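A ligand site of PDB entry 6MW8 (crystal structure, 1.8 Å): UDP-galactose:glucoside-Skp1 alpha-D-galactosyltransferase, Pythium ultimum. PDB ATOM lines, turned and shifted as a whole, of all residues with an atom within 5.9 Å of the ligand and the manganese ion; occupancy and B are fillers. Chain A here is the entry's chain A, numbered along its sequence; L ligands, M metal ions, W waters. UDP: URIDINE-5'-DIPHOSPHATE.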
ATOM      1  N   THR A  12      11.230 -30.243  26.213  1.00  0.00           N
ATOM      2  CA  THR A  12      12.205 -29.581  25.357  1.00  0.00           C
ATOM      3  C   THR A  12      12.279 -28.115  25.777  1.00  0.00           C
ATOM      4  O   THR A  12      11.598 -27.689  26.707  1.00  0.00           O
ATOM      5  CB  THR A  12      11.878 -29.784  23.871  1.00  0.00           C
ATOM      6  OG1 THR A  12      12.992 -29.356  23.051  1.00  0.00           O
ATOM      7  CG2 THR A  12      10.623 -29.052  23.448  1.00  0.00           C
ATOM      8  N   LEU A  13      13.153 -27.358  25.106  1.00  0.00           N
ATOM      9  CA  LEU A  13      13.484 -26.001  25.500  1.00  0.00           C
ATOM     10  C   LEU A  13      13.636 -25.124  24.270  1.00  0.00           C
ATOM     11  O   LEU A  13      14.247 -25.523  23.280  1.00  0.00           O
ATOM     12  CB  LEU A  13      14.798 -25.966  26.287  1.00  0.00           C
ATOM     13  CG  LEU A  13      15.359 -24.587  26.607  1.00  0.00           C
ATOM     14  CD1 LEU A  13      14.522 -23.891  27.678  1.00  0.00           C
ATOM     15  CD2 LEU A  13      16.801 -24.711  27.027  1.00  0.00           C
ATOM     16  N   ILE A  14      13.094 -23.906  24.349  1.00  0.00           N
ATOM     17  CA  ILE A  14      13.344 -22.894  23.338  1.00  0.00           C
ATOM     18  C   ILE A  14      13.737 -21.612  24.066  1.00  0.00           C
ATOM     19  O   ILE A  14      13.027 -21.161  24.975  1.00  0.00           O
ATOM     20  CB  ILE A  14      12.135 -22.680  22.417  1.00  0.00           C
ATOM     21  CG1 ILE A  14      12.409 -21.583  21.381  1.00  0.00           C
ATOM     22  CG2 ILE A  14      10.845 -22.412  23.208  1.00  0.00           C
ATOM     23  CD1 ILE A  14      11.387 -21.545  20.252  1.00  0.00           C
ATOM     24  N   THR A  15      14.911 -21.073  23.717  1.00  0.00           N
ATOM     25  CA  THR A  15      15.399 -19.824  24.306  1.00  0.00           C
ATOM     26  C   THR A  15      15.560 -18.714  23.266  1.00  0.00           C
ATOM     27  O   THR A  15      16.063 -17.639  23.598  1.00  0.00           O
ATOM     28  CB  THR A  15      16.726 -20.035  25.042  1.00  0.00           C
ATOM     29  OG1 THR A  15      17.713 -20.510  24.115  1.00  0.00           O
ATOM     30  CG2 THR A  15      16.580 -21.070  26.145  1.00  0.00           C
ATOM     31  N   SER A  16      15.146 -18.952  22.017  1.00  0.00           N
ATOM     32  CA  SER A  16      15.183 -17.930  20.992  1.00  0.00           C
ATOM     33  C   SER A  16      14.084 -18.205  19.973  1.00  0.00           C
ATOM     34  O   SER A  16      13.790 -19.369  19.674  1.00  0.00           O
ATOM     35  CB  SER A  16      16.535 -17.864  20.273  1.00  0.00           C
ATOM     36  OG  SER A  16      16.781 -19.054  19.554  1.00  0.00           O
ATOM     37  N   TYR A  19      14.616 -20.744  16.988  1.00  0.00           N
ATOM     38  CA  TYR A  19      14.575 -22.194  17.126  1.00  0.00           C
ATOM     39  C   TYR A  19      13.166 -22.761  17.076  1.00  0.00           C
ATOM     40  O   TYR A  19      12.973 -23.956  17.363  1.00  0.00           O
ATOM     41  CB  TYR A  19      15.252 -22.615  18.440  1.00  0.00           C
ATOM     42  CG  TYR A  19      16.736 -22.871  18.312  1.00  0.00           C
ATOM     43  CD1 TYR A  19      17.576 -21.913  17.770  1.00  0.00           C
ATOM     44  CD2 TYR A  19      17.300 -24.056  18.754  1.00  0.00           C
ATOM     45  CE1 TYR A  19      18.937 -22.129  17.652  1.00  0.00           C
ATOM     46  CE2 TYR A  19      18.674 -24.281  18.654  1.00  0.00           C
ATOM     47  CZ  TYR A  19      19.482 -23.306  18.102  1.00  0.00           C
ATOM     48  OH  TYR A  19      20.831 -23.508  17.989  1.00  0.00           O
ATOM     49  N   LYS A 101      18.799 -24.706  30.370  1.00  0.00           N
ATOM     50  CA  LYS A 101      18.432 -26.122  30.374  1.00  0.00           C
ATOM     51  C   LYS A 101      18.428 -26.723  31.783  1.00  0.00           C
ATOM     52  O   LYS A 101      17.675 -27.673  32.045  1.00  0.00           O
ATOM     53  CB  LYS A 101      19.409 -26.882  29.486  1.00  0.00           C
ATOM     54  CG  LYS A 101      19.179 -28.355  29.369  1.00  0.00           C
ATOM     55  CD  LYS A 101      20.310 -29.027  28.583  1.00  0.00           C
ATOM     56  CE  LYS A 101      20.406 -28.478  27.163  1.00  0.00           C
ATOM     57  NZ  LYS A 101      21.302 -29.308  26.308  1.00  0.00           N
ATOM     58  N   TYR A 115      14.491 -35.214  28.548  1.00  0.00           N
ATOM     59  CA  TYR A 115      14.760 -33.923  27.937  1.00  0.00           C
ATOM     60  C   TYR A 115      15.420 -34.153  26.582  1.00  0.00           C
ATOM     61  O   TYR A 115      16.380 -34.913  26.489  1.00  0.00           O
ATOM     62  CB  TYR A 115      15.677 -33.061  28.827  1.00  0.00           C
ATOM     63  CG  TYR A 115      16.167 -31.876  28.011  1.00  0.00           C
ATOM     64  CD1 TYR A 115      15.379 -30.751  27.849  1.00  0.00           C
ATOM     65  CD2 TYR A 115      17.395 -31.928  27.357  1.00  0.00           C
ATOM     66  CE1 TYR A 115      15.800 -29.698  27.037  1.00  0.00           C
ATOM     67  CE2 TYR A 115      17.822 -30.883  26.543  1.00  0.00           C
ATOM     68  CZ  TYR A 115      17.033 -29.779  26.401  1.00  0.00           C
ATOM     69  OH  TYR A 115      17.459 -28.748  25.586  1.00  0.00           O
ATOM     70  N   ILE A 116      14.926 -33.448  25.552  1.00  0.00           N
ATOM     71  CA  ILE A 116      15.496 -33.525  24.204  1.00  0.00           C
ATOM     72  C   ILE A 116      15.679 -32.113  23.660  1.00  0.00           C
ATOM     73  O   ILE A 116      14.706 -31.333  23.621  1.00  0.00           O
ATOM     74  CB  ILE A 116      14.625 -34.352  23.248  1.00  0.00           C
ATOM     75  CG1 ILE A 116      14.422 -35.777  23.778  1.00  0.00           C
ATOM     76  CG2 ILE A 116      15.252 -34.393  21.821  1.00  0.00           C
ATOM     77  CD1 ILE A 116      13.343 -36.545  22.998  1.00  0.00           C
ATOM     78  N   ASP A 117      16.905 -31.793  23.239  1.00  0.00           N
ATOM     79  CA  ASP A 117      17.201 -30.541  22.532  1.00  0.00           C
ATOM     80  C   ASP A 117      16.236 -30.278  21.376  1.00  0.00           C
ATOM     81  O   ASP A 117      15.823 -31.190  20.645  1.00  0.00           O
ATOM     82  CB  ASP A 117      18.621 -30.597  21.942  1.00  0.00           C
ATOM     83  CG  ASP A 117      19.715 -30.034  22.873  1.00  0.00           C
ATOM     84  OD1 ASP A 117      19.453 -29.722  24.051  1.00  0.00           O
ATOM     85  OD2 ASP A 117      20.863 -29.913  22.392  1.00  0.00           O
ATOM     86  N   ALA A 118      15.945 -28.994  21.146  1.00  0.00           N
ATOM     87  CA  ALA A 118      15.084 -28.623  20.025  1.00  0.00           C
ATOM     88  C   ALA A 118      15.744 -28.796  18.664  1.00  0.00           C
ATOM     89  O   ALA A 118      15.054 -28.657  17.654  1.00  0.00           O
ATOM     90  CB  ALA A 118      14.624 -27.164  20.176  1.00  0.00           C
ATOM     91  N   ASP A 119      17.044 -29.096  18.593  1.00  0.00           N
ATOM     92  CA  ASP A 119      17.668 -29.427  17.318  1.00  0.00           C
ATOM     93  C   ASP A 119      17.813 -30.941  17.119  1.00  0.00           C
ATOM     94  O   ASP A 119      18.698 -31.400  16.405  1.00  0.00           O
ATOM     95  CB  ASP A 119      19.038 -28.749  17.146  1.00  0.00           C
ATOM     96  CG  ASP A 119      20.063 -29.202  18.208  1.00  0.00           C
ATOM     97  OD1 ASP A 119      19.636 -29.573  19.304  1.00  0.00           O
ATOM     98  OD2 ASP A 119      21.296 -29.172  17.926  1.00  0.00           O
ATOM     99  N   ALA A 120      16.926 -31.716  17.730  1.00  0.00           N
ATOM    100  CA  ALA A 120      16.882 -33.149  17.491  1.00  0.00           C
ATOM    101  C   ALA A 120      15.512 -33.549  16.975  1.00  0.00           C
ATOM    102  O   ALA A 120      14.535 -32.796  17.083  1.00  0.00           O
ATOM    103  CB  ALA A 120      17.206 -33.950  18.760  1.00  0.00           C
ATOM    104  N   ASN A 149      27.133 -36.087  26.050  1.00  0.00           N
ATOM    105  CA  ASN A 149      26.512 -34.952  25.370  1.00  0.00           C
ATOM    106  C   ASN A 149      25.221 -34.597  26.105  1.00  0.00           C
ATOM    107  O   ASN A 149      24.510 -35.487  26.578  1.00  0.00           O
ATOM    108  CB  ASN A 149      26.206 -35.285  23.913  1.00  0.00           C
ATOM    109  CG  ASN A 149      25.560 -34.140  23.179  1.00  0.00           C
ATOM    110  OD1 ASN A 149      24.334 -34.076  23.085  1.00  0.00           O
ATOM    111  ND2 ASN A 149      26.371 -33.217  22.665  1.00  0.00           N
ATOM    112  N   GLY A 151      22.490 -33.146  24.970  1.00  0.00           N
ATOM    113  CA  GLY A 151      21.312 -32.923  24.144  1.00  0.00           C
ATOM    114  C   GLY A 151      20.136 -33.842  24.429  1.00  0.00           C
ATOM    115  O   GLY A 151      19.021 -33.548  23.997  1.00  0.00           O
ATOM    116  N   ASP A 176      33.798 -26.938  26.869  1.00  0.00           N
ATOM    117  CA  ASP A 176      33.256 -26.468  25.599  1.00  0.00           C
ATOM    118  C   ASP A 176      32.535 -25.126  25.733  1.00  0.00           C
ATOM    119  O   ASP A 176      31.914 -24.666  24.771  1.00  0.00           O
ATOM    120  CB  ASP A 176      32.337 -27.520  24.972  1.00  0.00           C
ATOM    121  CG  ASP A 176      30.982 -27.606  25.659  1.00  0.00           C
ATOM    122  OD1 ASP A 176      30.861 -27.193  26.828  1.00  0.00           O
ATOM    123  OD2 ASP A 176      30.034 -28.110  25.010  1.00  0.00           O
ATOM    124  N   ASP A 179      26.661 -25.869  28.205  1.00  0.00           N
ATOM    125  CA  ASP A 179      26.048 -26.710  29.228  1.00  0.00           C
ATOM    126  C   ASP A 179      26.653 -28.111  29.244  1.00  0.00           C
ATOM    127  O   ASP A 179      26.712 -28.743  30.304  1.00  0.00           O
ATOM    128  CB  ASP A 179      24.547 -26.792  29.015  1.00  0.00           C
ATOM    129  CG  ASP A 179      24.177 -27.259  27.623  1.00  0.00           C
ATOM    130  OD1 ASP A 179      24.516 -26.549  26.639  1.00  0.00           O
ATOM    131  OD2 ASP A 179      23.558 -28.332  27.508  1.00  0.00           O
ATOM    132  N   THR A 180      27.093 -28.617  28.082  1.00  0.00           N
ATOM    133  CA  THR A 180      27.722 -29.933  28.074  1.00  0.00           C
ATOM    134  C   THR A 180      29.000 -29.940  28.891  1.00  0.00           C
ATOM    135  O   THR A 180      29.218 -30.823  29.727  1.00  0.00           O
ATOM    136  CB  THR A 180      28.008 -30.384  26.639  1.00  0.00           C
ATOM    137  OG1 THR A 180      26.764 -30.582  25.946  1.00  0.00           O
ATOM    138  CG2 THR A 180      28.781 -31.685  26.638  1.00  0.00           C
ATOM    139  N   HIS A 231      20.400 -36.055  16.348  1.00  0.00           N
ATOM    140  CA  HIS A 231      20.708 -34.772  16.976  1.00  0.00           C
ATOM    141  C   HIS A 231      21.481 -33.910  15.986  1.00  0.00           C
ATOM    142  O   HIS A 231      22.599 -34.268  15.613  1.00  0.00           O
ATOM    143  CB  HIS A 231      21.494 -35.005  18.266  1.00  0.00           C
ATOM    144  CG  HIS A 231      21.773 -33.763  19.059  1.00  0.00           C
ATOM    145  ND1 HIS A 231      22.566 -33.770  20.191  1.00  0.00           N
ATOM    146  CD2 HIS A 231      21.370 -32.478  18.897  1.00  0.00           C
ATOM    147  CE1 HIS A 231      22.642 -32.535  20.682  1.00  0.00           C
ATOM    148  NE2 HIS A 231      21.935 -31.732  19.905  1.00  0.00           N
ATOM    149  N   TYR A 232      20.897 -32.783  15.579  1.00  0.00           N
ATOM    150  CA  TYR A 232      21.527 -31.908  14.584  1.00  0.00           C
ATOM    151  C   TYR A 232      22.460 -30.902  15.256  1.00  0.00           C
ATOM    152  O   TYR A 232      22.337 -29.685  15.094  1.00  0.00           O
ATOM    153  CB  TYR A 232      20.467 -31.229  13.736  1.00  0.00           C
ATOM    154  CG  TYR A 232      19.784 -32.215  12.846  1.00  0.00           C
ATOM    155  CD1 TYR A 232      18.812 -33.081  13.342  1.00  0.00           C
ATOM    156  CD2 TYR A 232      20.123 -32.318  11.498  1.00  0.00           C
ATOM    157  CE1 TYR A 232      18.194 -33.996  12.530  1.00  0.00           C
ATOM    158  CE2 TYR A 232      19.505 -33.233  10.687  1.00  0.00           C
ATOM    159  CZ  TYR A 232      18.560 -34.087  11.217  1.00  0.00           C
ATOM    160  OH  TYR A 232      17.939 -35.001  10.395  1.00  0.00           O
ATOM    161  N   SER A 233      23.413 -31.443  15.990  1.00  0.00           N
ATOM    162  CA  SER A 233      24.360 -30.616  16.700  1.00  0.00           C
ATOM    163  C   SER A 233      25.242 -29.852  15.711  1.00  0.00           C
ATOM    164  O   SER A 233      25.298 -30.162  14.517  1.00  0.00           O
ATOM    165  CB  SER A 233      25.217 -31.468  17.646  1.00  0.00           C
ATOM    166  OG  SER A 233      25.803 -32.560  16.960  1.00  0.00           O
ATOM    167  N   SER A 234      25.931 -28.850  16.252  1.00  0.00           N
ATOM    168  CA  SER A 234      26.774 -27.945  15.474  1.00  0.00           C
ATOM    169  C   SER A 234      25.944 -27.094  14.519  1.00  0.00           C
ATOM    170  O   SER A 234      24.710 -27.120  14.549  1.00  0.00           O
ATOM    171  CB  SER A 234      27.850 -28.715  14.711  1.00  0.00           C
ATOM    172  OG  SER A 234      28.798 -27.804  14.184  1.00  0.00           O
ATOM    173  N   ASN A 235      26.610 -26.313  13.686  1.00  0.00           N
ATOM    174  CA  ASN A 235      25.951 -25.239  12.963  1.00  0.00           C
ATOM    175  C   ASN A 235      26.308 -25.294  11.485  1.00  0.00           C
ATOM    176  O   ASN A 235      27.294 -25.929  11.097  1.00  0.00           O
ATOM    177  CB  ASN A 235      26.323 -23.880  13.575  1.00  0.00           C
ATOM    178  CG  ASN A 235      25.693 -23.688  14.959  1.00  0.00           C
ATOM    179  OD1 ASN A 235      24.562 -23.227  15.079  1.00  0.00           O
ATOM    180  ND2 ASN A 235      26.439 -24.064  16.001  1.00  0.00           N
ATOM    181  N   LYS A 237      22.120 -24.698  12.005  1.00  0.00           N
ATOM    182  CA  LYS A 237      20.997 -25.599  12.179  1.00  0.00           C
ATOM    183  C   LYS A 237      20.229 -25.741  10.861  1.00  0.00           C
ATOM    184  O   LYS A 237      20.273 -24.834  10.027  1.00  0.00           O
ATOM    185  CB  LYS A 237      20.078 -25.099  13.286  1.00  0.00           C
ATOM    186  CG  LYS A 237      20.804 -24.928  14.608  1.00  0.00           C
ATOM    187  CD  LYS A 237      21.425 -26.257  15.055  1.00  0.00           C
ATOM    188  CE  LYS A 237      22.076 -26.113  16.421  1.00  0.00           C
ATOM    189  NZ  LYS A 237      22.979 -27.243  16.735  1.00  0.00           N
HETATM  190  N1  UDP L   1      18.486 -23.170  22.339  1.00  0.00           N
HETATM  191  C2  UDP L   1      17.598 -22.305  21.751  1.00  0.00           C
HETATM  192  N3  UDP L   1      18.060 -21.217  21.065  1.00  0.00           N
HETATM  193  C4  UDP L   1      19.381 -20.999  20.945  1.00  0.00           C
HETATM  194  C5  UDP L   1      20.297 -21.902  21.552  1.00  0.00           C
HETATM  195  C6  UDP L   1      19.830 -22.954  22.242  1.00  0.00           C
HETATM  196  O2  UDP L   1      16.392 -22.484  21.858  1.00  0.00           O
HETATM  197  O4  UDP L   1      19.802 -20.040  20.327  1.00  0.00           O
HETATM  198  C1' UDP L   1      17.996 -24.330  23.082  1.00  0.00           C
HETATM  199  C2' UDP L   1      17.474 -25.426  22.124  1.00  0.00           C
HETATM  200  O2' UDP L   1      16.632 -26.342  22.817  1.00  0.00           O
HETATM  201  C3' UDP L   1      18.784 -26.119  21.774  1.00  0.00           C
HETATM  202  C4' UDP L   1      19.371 -26.236  23.177  1.00  0.00           C
HETATM  203  O4' UDP L   1      19.099 -24.956  23.804  1.00  0.00           O
HETATM  204  O3' UDP L   1      18.534 -27.401  21.211  1.00  0.00           O
HETATM  205  C5' UDP L   1      20.889 -26.505  23.132  1.00  0.00           C
HETATM  206  O5' UDP L   1      21.541 -25.654  22.181  1.00  0.00           O
HETATM  207  PA  UDP L   1      22.096 -26.247  20.808  1.00  0.00           P
HETATM  208  O1A UDP L   1      21.276 -27.420  20.426  1.00  0.00           O
HETATM  209  O2A UDP L   1      22.065 -25.139  19.683  1.00  0.00           O
HETATM  210  O3A UDP L   1      23.578 -26.731  21.015  1.00  0.00           O
HETATM  211  PB  UDP L   1      24.421 -27.878  20.347  1.00  0.00           P
HETATM  212  O1B UDP L   1      25.780 -28.029  21.151  1.00  0.00           O
HETATM  213  O2B UDP L   1      24.694 -27.518  18.848  1.00  0.00           O
HETATM  214  O3B UDP L   1      23.643 -29.150  20.399  1.00  0.00           O
HETATM  215 MN    MN M   1      21.593 -29.609  20.268  1.00  0.00          MN
HETATM  216  O   HOH W   1      18.918 -18.584  17.762  1.00  0.00           O
HETATM  217  O   HOH W   2      27.368 -29.771  23.229  1.00  0.00           O
HETATM  218  O   HOH W   3      25.837 -25.142  18.333  1.00  0.00           O
HETATM  219  O   HOH W   4      24.247 -27.556  24.234  1.00  0.00           O
HETATM  220  O   HOH W   5      25.325 -30.821  21.755  1.00  0.00           O
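The backbone NH of Asp 119 is in hydrogen-bond range of an oxygen (O3') of the ligand (3.5 Å). The backbone carbonyl oxygen of Leu 13 is in hydrogen-bond range of an oxygen (O2') of the ligand. The side-chain hydroxyl of Tyr 19 sits at hydrogen-bond distance from an oxygen (O2A) of the ligand (2.7 Å). N of Ala 118 lies within hydrogen-bond range of O3' of the ligand. The side-chain hydroxyl (OG) of Ser 16 is in hydrogen-bond range of a nitrogen (N3) of the ligand (2.9 Å). N3 of the ligand sits close to OG1 of Thr 15 (3.2 Å). N of Thr 15 sits at hydrogen-bond distance from O2 of the ligand, at 2.8 Å. NZ of Lys 237 is in salt-bridge range of O2B of the ligand. The backbone NH (N) of Ser 234 is in hydrogen-bond range of an oxygen (O2B) of the ligand (3.2 Å).
The side-chain amino group (NZ) of Lys 237 sits at hydrogen-bond distance from the backbone carbonyl oxygen (O) of Tyr 232 (3.0 Å). The backbone NH (N) of Tyr 232 lies within hydrogen-bond range of the backbone carbonyl oxygen (O) of Asp 119, 2.7 Å away. The side-chain carboxylate (OD2) of Asp 119 sits close to the side-chain amino group (NZ) of Lys 237. O of Gly 151 sits at hydrogen-bond distance from N of Asp 117. ND1 of His 231 sits close to OD1 of Asn 149 (3.4 Å). OH of Tyr 115 is in hydrogen-bond range of OD1 of Asp 117 (2.7 Å). The side-chain amino group (NZ) of Lys 237 is in hydrogen-bond range of the backbone carbonyl oxygen (O) of Ser 234 (2.8 Å). The side-chain amino group of Lys 101 is in salt-bridge range of the side-chain carboxylate of Asp 117 (2.9 Å).
Ile 14 touches the ligand. Tyr 115 touches the ligand (OH to O2', 3.8 Å). Ser 233 touches the ligand. Hydrophobic or aromatic side chains that line the ligand: Leu 13, Tyr 19, Ala 118 and His 231. Within 4 Å of the ligand: Leu 13, Ile 14, Thr 15, Ser 16, Tyr 19, Tyr 115, Asp 117, Ala 118, Asp 119, His 231, Ser 233, Ser 234 and Lys 237. The nearest printed residue that does not touch the ligand is Lys 101 (4.3 Å).
Within 4 Å of the manganese ion: Asp 117, Asp 119 and His 231. The nearest printed residue that does not touch the manganese ion is Lys 237 (4.5 Å).
The manganese ion is bound by an oxygen (O3B) of the ligand, a ring nitrogen (NE2) of His 231, the side-chain carboxylate (OD1) of Asp 119, an oxygen (O1A) of the ligand, the side-chain carboxylate (OD2) of Asp 117 and the side-chain carboxylate (OD2) of Asp 119. The manganese ion has six donor atoms within binding distance.
Water W3 lies within hydrogen-bond range of the side-chain amide nitrogen of Asn 235 (2.6 Å) and an oxygen (O2B) of the ligand (2.7 Å). Water W5 lies within hydrogen-bond range of the side-chain amide nitrogen of Asn 149 and an oxygen (O1B) of the ligand. Water W1 lies within hydrogen-bond range of OG of Ser 16 (2.8 Å) and O4 of the ligand (3.1 Å). Water W2 lies within hydrogen-bond range of the side-chain hydroxyl (OG1) of Thr 180 (2.9 Å) and an oxygen (O1B) of the ligand (3.1 Å). Water W4 bridges OD1 of Asp 179 (2.6 Å) and O3A of the ligand (3.4 Å).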
